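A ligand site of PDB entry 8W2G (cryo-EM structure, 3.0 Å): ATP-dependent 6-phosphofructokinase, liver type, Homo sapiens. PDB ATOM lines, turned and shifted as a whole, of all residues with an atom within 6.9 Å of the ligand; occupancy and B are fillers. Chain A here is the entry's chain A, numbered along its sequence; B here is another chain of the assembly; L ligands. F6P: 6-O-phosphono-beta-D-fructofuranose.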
ATOM      1  N   GLY A  24     -23.554 -14.164   6.233  1.00  0.00           N
ATOM      2  CA  GLY A  24     -23.998 -14.324   7.593  1.00  0.00           C
ATOM      3  C   GLY A  24     -22.865 -14.134   8.590  1.00  0.00           C
ATOM      4  O   GLY A  24     -21.796 -13.598   8.271  1.00  0.00           O
ATOM      5  N   GLY A  25     -23.122 -14.574   9.823  1.00  0.00           N
ATOM      6  CA  GLY A  25     -22.127 -14.488  10.873  1.00  0.00           C
ATOM      7  C   GLY A  25     -20.922 -15.350  10.562  1.00  0.00           C
ATOM      8  O   GLY A  25     -21.051 -16.552  10.323  1.00  0.00           O
ATOM      9  N   ASP A  26     -19.735 -14.749  10.550  1.00  0.00           N
ATOM     10  CA  ASP A  26     -18.538 -15.481  10.197  1.00  0.00           C
ATOM     11  C   ASP A  26     -18.203 -16.497  11.277  1.00  0.00           C
ATOM     12  O   ASP A  26     -18.645 -16.383  12.429  1.00  0.00           O
ATOM     13  CB  ASP A  26     -17.364 -14.536   9.970  1.00  0.00           C
ATOM     14  CG  ASP A  26     -16.917 -13.848  11.242  1.00  0.00           C
ATOM     15  OD1 ASP A  26     -17.724 -13.707  12.187  1.00  0.00           O
ATOM     16  OD2 ASP A  26     -15.740 -13.445  11.291  1.00  0.00           O
ATOM     17  N   ARG A  88     -23.493  -8.028   5.112  1.00  0.00           N
ATOM     18  CA  ARG A  88     -24.917  -8.254   4.980  1.00  0.00           C
ATOM     19  C   ARG A  88     -25.500  -7.330   3.909  1.00  0.00           C
ATOM     20  O   ARG A  88     -25.037  -6.198   3.738  1.00  0.00           O
ATOM     21  CB  ARG A  88     -25.643  -8.030   6.309  1.00  0.00           C
ATOM     22  CG  ARG A  88     -26.832  -8.947   6.510  1.00  0.00           C
ATOM     23  CD  ARG A  88     -27.654  -8.577   7.733  1.00  0.00           C
ATOM     24  NE  ARG A  88     -27.036  -9.050   8.975  1.00  0.00           N
ATOM     25  CZ  ARG A  88     -26.840  -8.347  10.093  1.00  0.00           C
ATOM     26  NH1 ARG A  88     -27.206  -7.086  10.204  1.00  0.00           N
ATOM     27  NH2 ARG A  88     -26.261  -8.947  11.128  1.00  0.00           N
ATOM     28  N   SER A 164     -21.388 -21.673  10.973  1.00  0.00           N
ATOM     29  CA  SER A 164     -22.003 -21.029  12.125  1.00  0.00           C
ATOM     30  C   SER A 164     -21.517 -21.704  13.387  1.00  0.00           C
ATOM     31  O   SER A 164     -21.385 -22.932  13.426  1.00  0.00           O
ATOM     32  CB  SER A 164     -23.541 -21.117  12.043  1.00  0.00           C
ATOM     33  OG  SER A 164     -24.143 -20.490  13.159  1.00  0.00           O
ATOM     34  N   ILE A 165     -21.253 -20.907  14.426  1.00  0.00           N
ATOM     35  CA  ILE A 165     -20.827 -21.465  15.708  1.00  0.00           C
ATOM     36  C   ILE A 165     -21.983 -22.037  16.518  1.00  0.00           C
ATOM     37  O   ILE A 165     -21.749 -22.756  17.490  1.00  0.00           O
ATOM     38  CB  ILE A 165     -20.047 -20.415  16.530  1.00  0.00           C
ATOM     39  CG1 ILE A 165     -20.914 -19.225  17.029  1.00  0.00           C
ATOM     40  CG2 ILE A 165     -18.891 -19.849  15.699  1.00  0.00           C
ATOM     41  CD1 ILE A 165     -20.270 -18.469  18.163  1.00  0.00           C
ATOM     42  N   ASP A 166     -23.230 -21.720  16.140  1.00  0.00           N
ATOM     43  CA  ASP A 166     -24.367 -22.075  16.982  1.00  0.00           C
ATOM     44  C   ASP A 166     -24.658 -23.570  16.905  1.00  0.00           C
ATOM     45  O   ASP A 166     -25.021 -24.182  17.914  1.00  0.00           O
ATOM     46  CB  ASP A 166     -25.597 -21.279  16.557  1.00  0.00           C
ATOM     47  CG  ASP A 166     -25.327 -19.795  16.450  1.00  0.00           C
ATOM     48  OD1 ASP A 166     -24.474 -19.289  17.202  1.00  0.00           O
ATOM     49  OD2 ASP A 166     -25.965 -19.133  15.596  1.00  0.00           O
ATOM     50  N   VAL A 207     -22.668 -17.455  27.257  1.00  0.00           N
ATOM     51  CA  VAL A 207     -22.122 -17.992  26.011  1.00  0.00           C
ATOM     52  C   VAL A 207     -23.076 -17.623  24.884  1.00  0.00           C
ATOM     53  O   VAL A 207     -24.274 -17.416  25.098  1.00  0.00           O
ATOM     54  CB  VAL A 207     -21.924 -19.528  26.116  1.00  0.00           C
ATOM     55  CG1 VAL A 207     -21.169 -20.060  24.900  1.00  0.00           C
ATOM     56  CG2 VAL A 207     -21.190 -19.905  27.409  1.00  0.00           C
ATOM     57  N   MET A 208     -22.547 -17.555  23.664  1.00  0.00           N
ATOM     58  CA  MET A 208     -23.361 -17.276  22.499  1.00  0.00           C
ATOM     59  C   MET A 208     -24.131 -18.536  22.114  1.00  0.00           C
ATOM     60  O   MET A 208     -24.156 -19.526  22.856  1.00  0.00           O
ATOM     61  CB  MET A 208     -22.490 -16.723  21.368  1.00  0.00           C
ATOM     62  CG  MET A 208     -21.916 -15.348  21.652  1.00  0.00           C
ATOM     63  SD  MET A 208     -20.588 -14.898  20.525  1.00  0.00           S
ATOM     64  CE  MET A 208     -21.484 -14.725  18.986  1.00  0.00           C
ATOM     65  N   GLY A 209     -24.769 -18.521  20.942  1.00  0.00           N
ATOM     66  CA  GLY A 209     -25.783 -19.493  20.577  1.00  0.00           C
ATOM     67  C   GLY A 209     -27.097 -18.756  20.515  1.00  0.00           C
ATOM     68  O   GLY A 209     -27.678 -18.445  21.554  1.00  0.00           O
ATOM     69  N   ARG A 210     -27.553 -18.458  19.291  1.00  0.00           N
ATOM     70  CA  ARG A 210     -28.629 -17.502  19.073  1.00  0.00           C
ATOM     71  C   ARG A 210     -29.903 -17.918  19.806  1.00  0.00           C
ATOM     72  O   ARG A 210     -30.383 -17.211  20.694  1.00  0.00           O
ATOM     73  CB  ARG A 210     -28.881 -17.351  17.564  1.00  0.00           C
ATOM     74  CG  ARG A 210     -29.376 -15.965  17.122  1.00  0.00           C
ATOM     75  CD  ARG A 210     -29.109 -15.721  15.634  1.00  0.00           C
ATOM     76  NE  ARG A 210     -29.168 -14.303  15.287  1.00  0.00           N
ATOM     77  CZ  ARG A 210     -30.269 -13.622  15.030  1.00  0.00           C
ATOM     78  NH1 ARG A 210     -31.474 -14.177  15.079  1.00  0.00           N
ATOM     79  NH2 ARG A 210     -30.178 -12.331  14.716  1.00  0.00           N
ATOM     80  N   HIS A 211     -30.454 -19.071  19.445  1.00  0.00           N
ATOM     81  CA  HIS A 211     -31.595 -19.678  20.112  1.00  0.00           C
ATOM     82  C   HIS A 211     -31.312 -21.163  20.388  1.00  0.00           C
ATOM     83  O   HIS A 211     -32.231 -21.967  20.486  1.00  0.00           O
ATOM     84  CB  HIS A 211     -32.866 -19.511  19.287  1.00  0.00           C
ATOM     85  CG  HIS A 211     -33.390 -18.103  19.230  1.00  0.00           C
ATOM     86  ND1 HIS A 211     -32.631 -17.039  18.791  1.00  0.00           N
ATOM     87  CD2 HIS A 211     -34.605 -17.588  19.550  1.00  0.00           C
ATOM     88  CE1 HIS A 211     -33.344 -15.927  18.862  1.00  0.00           C
ATOM     89  NE2 HIS A 211     -34.550 -16.241  19.312  1.00  0.00           N
ATOM     90  N   LEU A 215     -23.727 -24.874  22.407  1.00  0.00           N
ATOM     91  CA  LEU A 215     -22.482 -24.338  22.950  1.00  0.00           C
ATOM     92  C   LEU A 215     -22.482 -24.359  24.464  1.00  0.00           C
ATOM     93  O   LEU A 215     -21.481 -24.742  25.094  1.00  0.00           O
ATOM     94  CB  LEU A 215     -22.261 -22.909  22.457  1.00  0.00           C
ATOM     95  CG  LEU A 215     -21.986 -22.657  20.976  1.00  0.00           C
ATOM     96  CD1 LEU A 215     -21.898 -21.161  20.734  1.00  0.00           C
ATOM     97  CD2 LEU A 215     -20.702 -23.349  20.527  1.00  0.00           C
ATOM     98  N   GLU A 264     -27.237 -17.305  25.666  1.00  0.00           N
ATOM     99  CA  GLU A 264     -27.791 -15.973  25.428  1.00  0.00           C
ATOM    100  C   GLU A 264     -29.253 -15.992  25.008  1.00  0.00           C
ATOM    101  O   GLU A 264     -29.847 -14.916  24.866  1.00  0.00           O
ATOM    102  CB  GLU A 264     -26.954 -15.229  24.381  1.00  0.00           C
ATOM    103  CG  GLU A 264     -26.981 -15.813  22.974  1.00  0.00           C
ATOM    104  CD  GLU A 264     -26.145 -15.000  22.000  1.00  0.00           C
ATOM    105  OE1 GLU A 264     -25.644 -13.929  22.391  1.00  0.00           O
ATOM    106  OE2 GLU A 264     -25.990 -15.442  20.842  1.00  0.00           O
ATOM    107  N   HIS A 298     -17.981 -11.579  21.408  1.00  0.00           N
ATOM    108  CA  HIS A 298     -17.503 -11.960  20.077  1.00  0.00           C
ATOM    109  C   HIS A 298     -16.098 -12.600  20.083  1.00  0.00           C
ATOM    110  O   HIS A 298     -15.501 -12.749  19.003  1.00  0.00           O
ATOM    111  CB  HIS A 298     -17.508 -10.724  19.171  1.00  0.00           C
ATOM    112  CG  HIS A 298     -18.885 -10.325  18.732  1.00  0.00           C
ATOM    113  ND1 HIS A 298     -19.939 -10.187  19.609  1.00  0.00           N
ATOM    114  CD2 HIS A 298     -19.379 -10.040  17.502  1.00  0.00           C
ATOM    115  CE1 HIS A 298     -21.018  -9.823  18.944  1.00  0.00           C
ATOM    116  NE2 HIS A 298     -20.714  -9.732  17.668  1.00  0.00           N
ATOM    117  N   GLN A 300     -15.816 -15.666  20.731  1.00  0.00           N
ATOM    118  CA  GLN A 300     -16.173 -16.965  20.163  1.00  0.00           C
ATOM    119  C   GLN A 300     -16.139 -16.967  18.648  1.00  0.00           C
ATOM    120  O   GLN A 300     -15.910 -18.014  18.029  1.00  0.00           O
ATOM    121  CB  GLN A 300     -17.554 -17.360  20.658  1.00  0.00           C
ATOM    122  CG  GLN A 300     -17.598 -17.681  22.130  1.00  0.00           C
ATOM    123  CD  GLN A 300     -18.911 -17.347  22.779  1.00  0.00           C
ATOM    124  OE1 GLN A 300     -19.891 -18.064  22.631  1.00  0.00           O
ATOM    125  NE2 GLN A 300     -18.941 -16.250  23.525  1.00  0.00           N
ATOM    126  N   ARG A 301     -16.370 -15.816  18.018  1.00  0.00           N
ATOM    127  CA  ARG A 301     -16.453 -15.725  16.565  1.00  0.00           C
ATOM    128  C   ARG A 301     -15.104 -15.592  15.873  1.00  0.00           C
ATOM    129  O   ARG A 301     -15.083 -15.500  14.638  1.00  0.00           O
ATOM    130  CB  ARG A 301     -17.333 -14.536  16.184  1.00  0.00           C
ATOM    131  CG  ARG A 301     -18.811 -14.752  16.466  1.00  0.00           C
ATOM    132  CD  ARG A 301     -19.557 -15.321  15.271  1.00  0.00           C
ATOM    133  NE  ARG A 301     -19.602 -14.384  14.150  1.00  0.00           N
ATOM    134  CZ  ARG A 301     -20.358 -13.289  14.099  1.00  0.00           C
ATOM    135  NH1 ARG A 301     -21.201 -12.969  15.075  1.00  0.00           N
ATOM    136  NH2 ARG A 301     -20.273 -12.497  13.029  1.00  0.00           N
ATOM    137  N   THR B 195     -12.870 -11.389  13.391  1.00  0.00           N
ATOM    138  CA  THR B 195     -14.269 -11.109  13.102  1.00  0.00           C
ATOM    139  C   THR B 195     -14.516  -9.632  12.834  1.00  0.00           C
ATOM    140  O   THR B 195     -15.375  -9.282  12.014  1.00  0.00           O
ATOM    141  CB  THR B 195     -15.179 -11.610  14.236  1.00  0.00           C
ATOM    142  OG1 THR B 195     -16.547 -11.337  13.903  1.00  0.00           O
ATOM    143  CG2 THR B 195     -14.846 -10.959  15.593  1.00  0.00           C
ATOM    144  N   HIS B 199     -16.163  -8.443   9.261  1.00  0.00           N
ATOM    145  CA  HIS B 199     -17.444  -7.763   9.156  1.00  0.00           C
ATOM    146  C   HIS B 199     -17.338  -6.243   9.098  1.00  0.00           C
ATOM    147  O   HIS B 199     -18.371  -5.577   8.954  1.00  0.00           O
ATOM    148  CB  HIS B 199     -18.340  -8.163  10.336  1.00  0.00           C
ATOM    149  CG  HIS B 199     -19.167  -9.381  10.067  1.00  0.00           C
ATOM    150  ND1 HIS B 199     -20.397  -9.323   9.443  1.00  0.00           N
ATOM    151  CD2 HIS B 199     -18.934 -10.694  10.315  1.00  0.00           C
ATOM    152  CE1 HIS B 199     -20.888 -10.535   9.338  1.00  0.00           C
ATOM    153  NE2 HIS B 199     -20.019 -11.387   9.855  1.00  0.00           N
ATOM    154  N   ARG B 201     -16.322  -3.989  11.558  1.00  0.00           N
ATOM    155  CA  ARG B 201     -17.004  -3.566  12.771  1.00  0.00           C
ATOM    156  C   ARG B 201     -16.053  -2.844  13.707  1.00  0.00           C
ATOM    157  O   ARG B 201     -14.898  -3.231  13.865  1.00  0.00           O
ATOM    158  CB  ARG B 201     -17.604  -4.759  13.495  1.00  0.00           C
ATOM    159  CG  ARG B 201     -18.931  -5.230  12.949  1.00  0.00           C
ATOM    160  CD  ARG B 201     -19.398  -6.418  13.741  1.00  0.00           C
ATOM    161  NE  ARG B 201     -20.572  -7.079  13.184  1.00  0.00           N
ATOM    162  CZ  ARG B 201     -21.090  -8.211  13.642  1.00  0.00           C
ATOM    163  NH1 ARG B 201     -20.564  -8.834  14.686  1.00  0.00           N
ATOM    164  NH2 ARG B 201     -22.161  -8.716  13.044  1.00  0.00           N
ATOM    165  N   PHE B 203     -15.116  -1.941  17.598  1.00  0.00           N
ATOM    166  CA  PHE B 203     -15.203  -2.683  18.849  1.00  0.00           C
ATOM    167  C   PHE B 203     -14.733  -1.799  19.991  1.00  0.00           C
ATOM    168  O   PHE B 203     -13.746  -1.061  19.858  1.00  0.00           O
ATOM    169  CB  PHE B 203     -14.374  -3.963  18.802  1.00  0.00           C
ATOM    170  CG  PHE B 203     -15.133  -5.174  18.306  1.00  0.00           C
ATOM    171  CD1 PHE B 203     -15.863  -5.958  19.187  1.00  0.00           C
ATOM    172  CD2 PHE B 203     -15.108  -5.515  16.971  1.00  0.00           C
ATOM    173  CE1 PHE B 203     -16.558  -7.066  18.729  1.00  0.00           C
ATOM    174  CE2 PHE B 203     -15.811  -6.618  16.515  1.00  0.00           C
ATOM    175  CZ  PHE B 203     -16.536  -7.393  17.394  1.00  0.00           C
ATOM    176  N   ASP B 290     -21.433  -0.167  12.292  1.00  0.00           N
ATOM    177  CA  ASP B 290     -21.802  -1.318  13.100  1.00  0.00           C
ATOM    178  C   ASP B 290     -20.723  -1.534  14.146  1.00  0.00           C
ATOM    179  O   ASP B 290     -19.533  -1.557  13.814  1.00  0.00           O
ATOM    180  CB  ASP B 290     -21.955  -2.562  12.221  1.00  0.00           C
ATOM    181  CG  ASP B 290     -22.585  -3.732  12.956  1.00  0.00           C
ATOM    182  OD1 ASP B 290     -23.236  -3.511  13.991  1.00  0.00           O
ATOM    183  OD2 ASP B 290     -22.426  -4.877  12.493  1.00  0.00           O
ATOM    184  N   THR B 291     -21.138  -1.692  15.400  1.00  0.00           N
ATOM    185  CA  THR B 291     -20.197  -1.725  16.514  1.00  0.00           C
ATOM    186  C   THR B 291     -20.674  -2.676  17.582  1.00  0.00           C
ATOM    187  O   THR B 291     -21.847  -3.054  17.638  1.00  0.00           O
ATOM    188  CB  THR B 291     -19.969  -0.327  17.096  1.00  0.00           C
ATOM    189  OG1 THR B 291     -19.016  -0.392  18.163  1.00  0.00           O
ATOM    190  CG2 THR B 291     -21.270   0.273  17.617  1.00  0.00           C
ATOM    191  N   ARG B 292     -19.741  -3.059  18.461  1.00  0.00           N
ATOM    192  CA  ARG B 292     -20.021  -3.915  19.593  1.00  0.00           C
ATOM    193  C   ARG B 292     -19.169  -3.470  20.763  1.00  0.00           C
ATOM    194  O   ARG B 292     -18.267  -2.632  20.617  1.00  0.00           O
ATOM    195  CB  ARG B 292     -19.742  -5.397  19.263  1.00  0.00           C
ATOM    196  CG  ARG B 292     -20.622  -6.008  18.181  1.00  0.00           C
ATOM    197  CD  ARG B 292     -22.078  -6.126  18.614  1.00  0.00           C
ATOM    198  NE  ARG B 292     -22.921  -6.711  17.582  1.00  0.00           N
ATOM    199  CZ  ARG B 292     -23.306  -6.089  16.465  1.00  0.00           C
ATOM    200  NH1 ARG B 292     -22.911  -4.856  16.178  1.00  0.00           N
ATOM    201  NH2 ARG B 292     -24.115  -6.720  15.624  1.00  0.00           N
HETATM  202  O1  F6P L   1     -24.466 -15.342  14.000  1.00  0.00           O
HETATM  203  C1  F6P L   1     -24.563 -16.348  15.015  1.00  0.00           C
HETATM  204  C2  F6P L   1     -23.928 -15.794  16.294  1.00  0.00           C
HETATM  205  O2  F6P L   1     -22.720 -16.465  16.576  1.00  0.00           O
HETATM  206  C3  F6P L   1     -24.924 -15.940  17.496  1.00  0.00           C
HETATM  207  O3  F6P L   1     -24.374 -16.671  18.469  1.00  0.00           O
HETATM  208  C4  F6P L   1     -25.170 -14.459  17.995  1.00  0.00           C
HETATM  209  O4  F6P L   1     -26.535 -14.306  18.474  1.00  0.00           O
HETATM  210  C5  F6P L   1     -25.005 -13.783  16.919  1.00  0.00           C
HETATM  211  O5  F6P L   1     -23.728 -14.514  16.164  1.00  0.00           O
HETATM  212  C6  F6P L   1     -24.650 -12.331  17.229  1.00  0.00           C
HETATM  213  O6  F6P L   1     -24.239 -11.780  16.012  1.00  0.00           O
HETATM  214  P   F6P L   1     -23.811 -10.163  15.962  1.00  0.00           P
HETATM  215  O1P F6P L   1     -24.233  -9.478  17.244  1.00  0.00           O
HETATM  216  O2P F6P L   1     -24.459  -9.520  14.824  1.00  0.00           O
HETATM  217  O3P F6P L   1     -22.325 -10.066  15.806  1.00  0.00           O
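The guanidinium group (NE) of Arg 201 of chain B is in salt-bridge range of the side-chain carboxylate (OD2) of Asp 290 of chain B (3.0 Å). OD1 of Asp 26 is in salt-bridge range of NE of Arg 301, 2.8 Å away. NH1 of Arg 201 of chain B is in hydrogen-bond range of NE2 of His 298. OE1 of Gln 300 lies within hydrogen-bond range of N of Met 208 (2.9 Å). The side-chain carboxylate (OE2) of Glu 264 sits at hydrogen-bond distance from the backbone NH (N) of Gly 209 (3.3 Å). The side-chain carboxylate of Asp 166 lies within hydrogen-bond range of the side-chain hydroxyl of Ser 164 (3.3 Å). The backbone NH (N) of Glu 264 is in hydrogen-bond range of the backbone carbonyl oxygen (O) of Val 207. The guanidinium group of Arg 301 lies within hydrogen-bond range of a ring nitrogen (NE2) of His 199 of chain B.
NH2 of Arg 292 of chain B is in salt-bridge range of O2P of the ligand (2.9 Å). A ring nitrogen (NE2) of His 298 is in hydrogen-bond range of an oxygen (O3P) of the ligand (2.5 Å). O3 of the ligand lies within hydrogen-bond range of N of Gly 209 (3.1 Å). NH1 of Arg 201 of chain B lies within salt-bridge range of O3P of the ligand (2.4 Å). The side-chain carboxylate (OE2) of Glu 264 lies within hydrogen-bond range of an oxygen (O4) of the ligand, at 2.7 Å. The side-chain carboxylate (OD1) of Asp 166 sits at hydrogen-bond distance from an oxygen (O3) of the ligand (2.9 Å). The guanidinium group (NH1) of Arg 301 lies within salt-bridge range of an oxygen (O3P) of the ligand.
Residues that only touch the ligand: Gly 25, Ile 165, Met 208 and Arg 210. Of the 24 residues printed, 11 come within 4 Å of the ligand.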
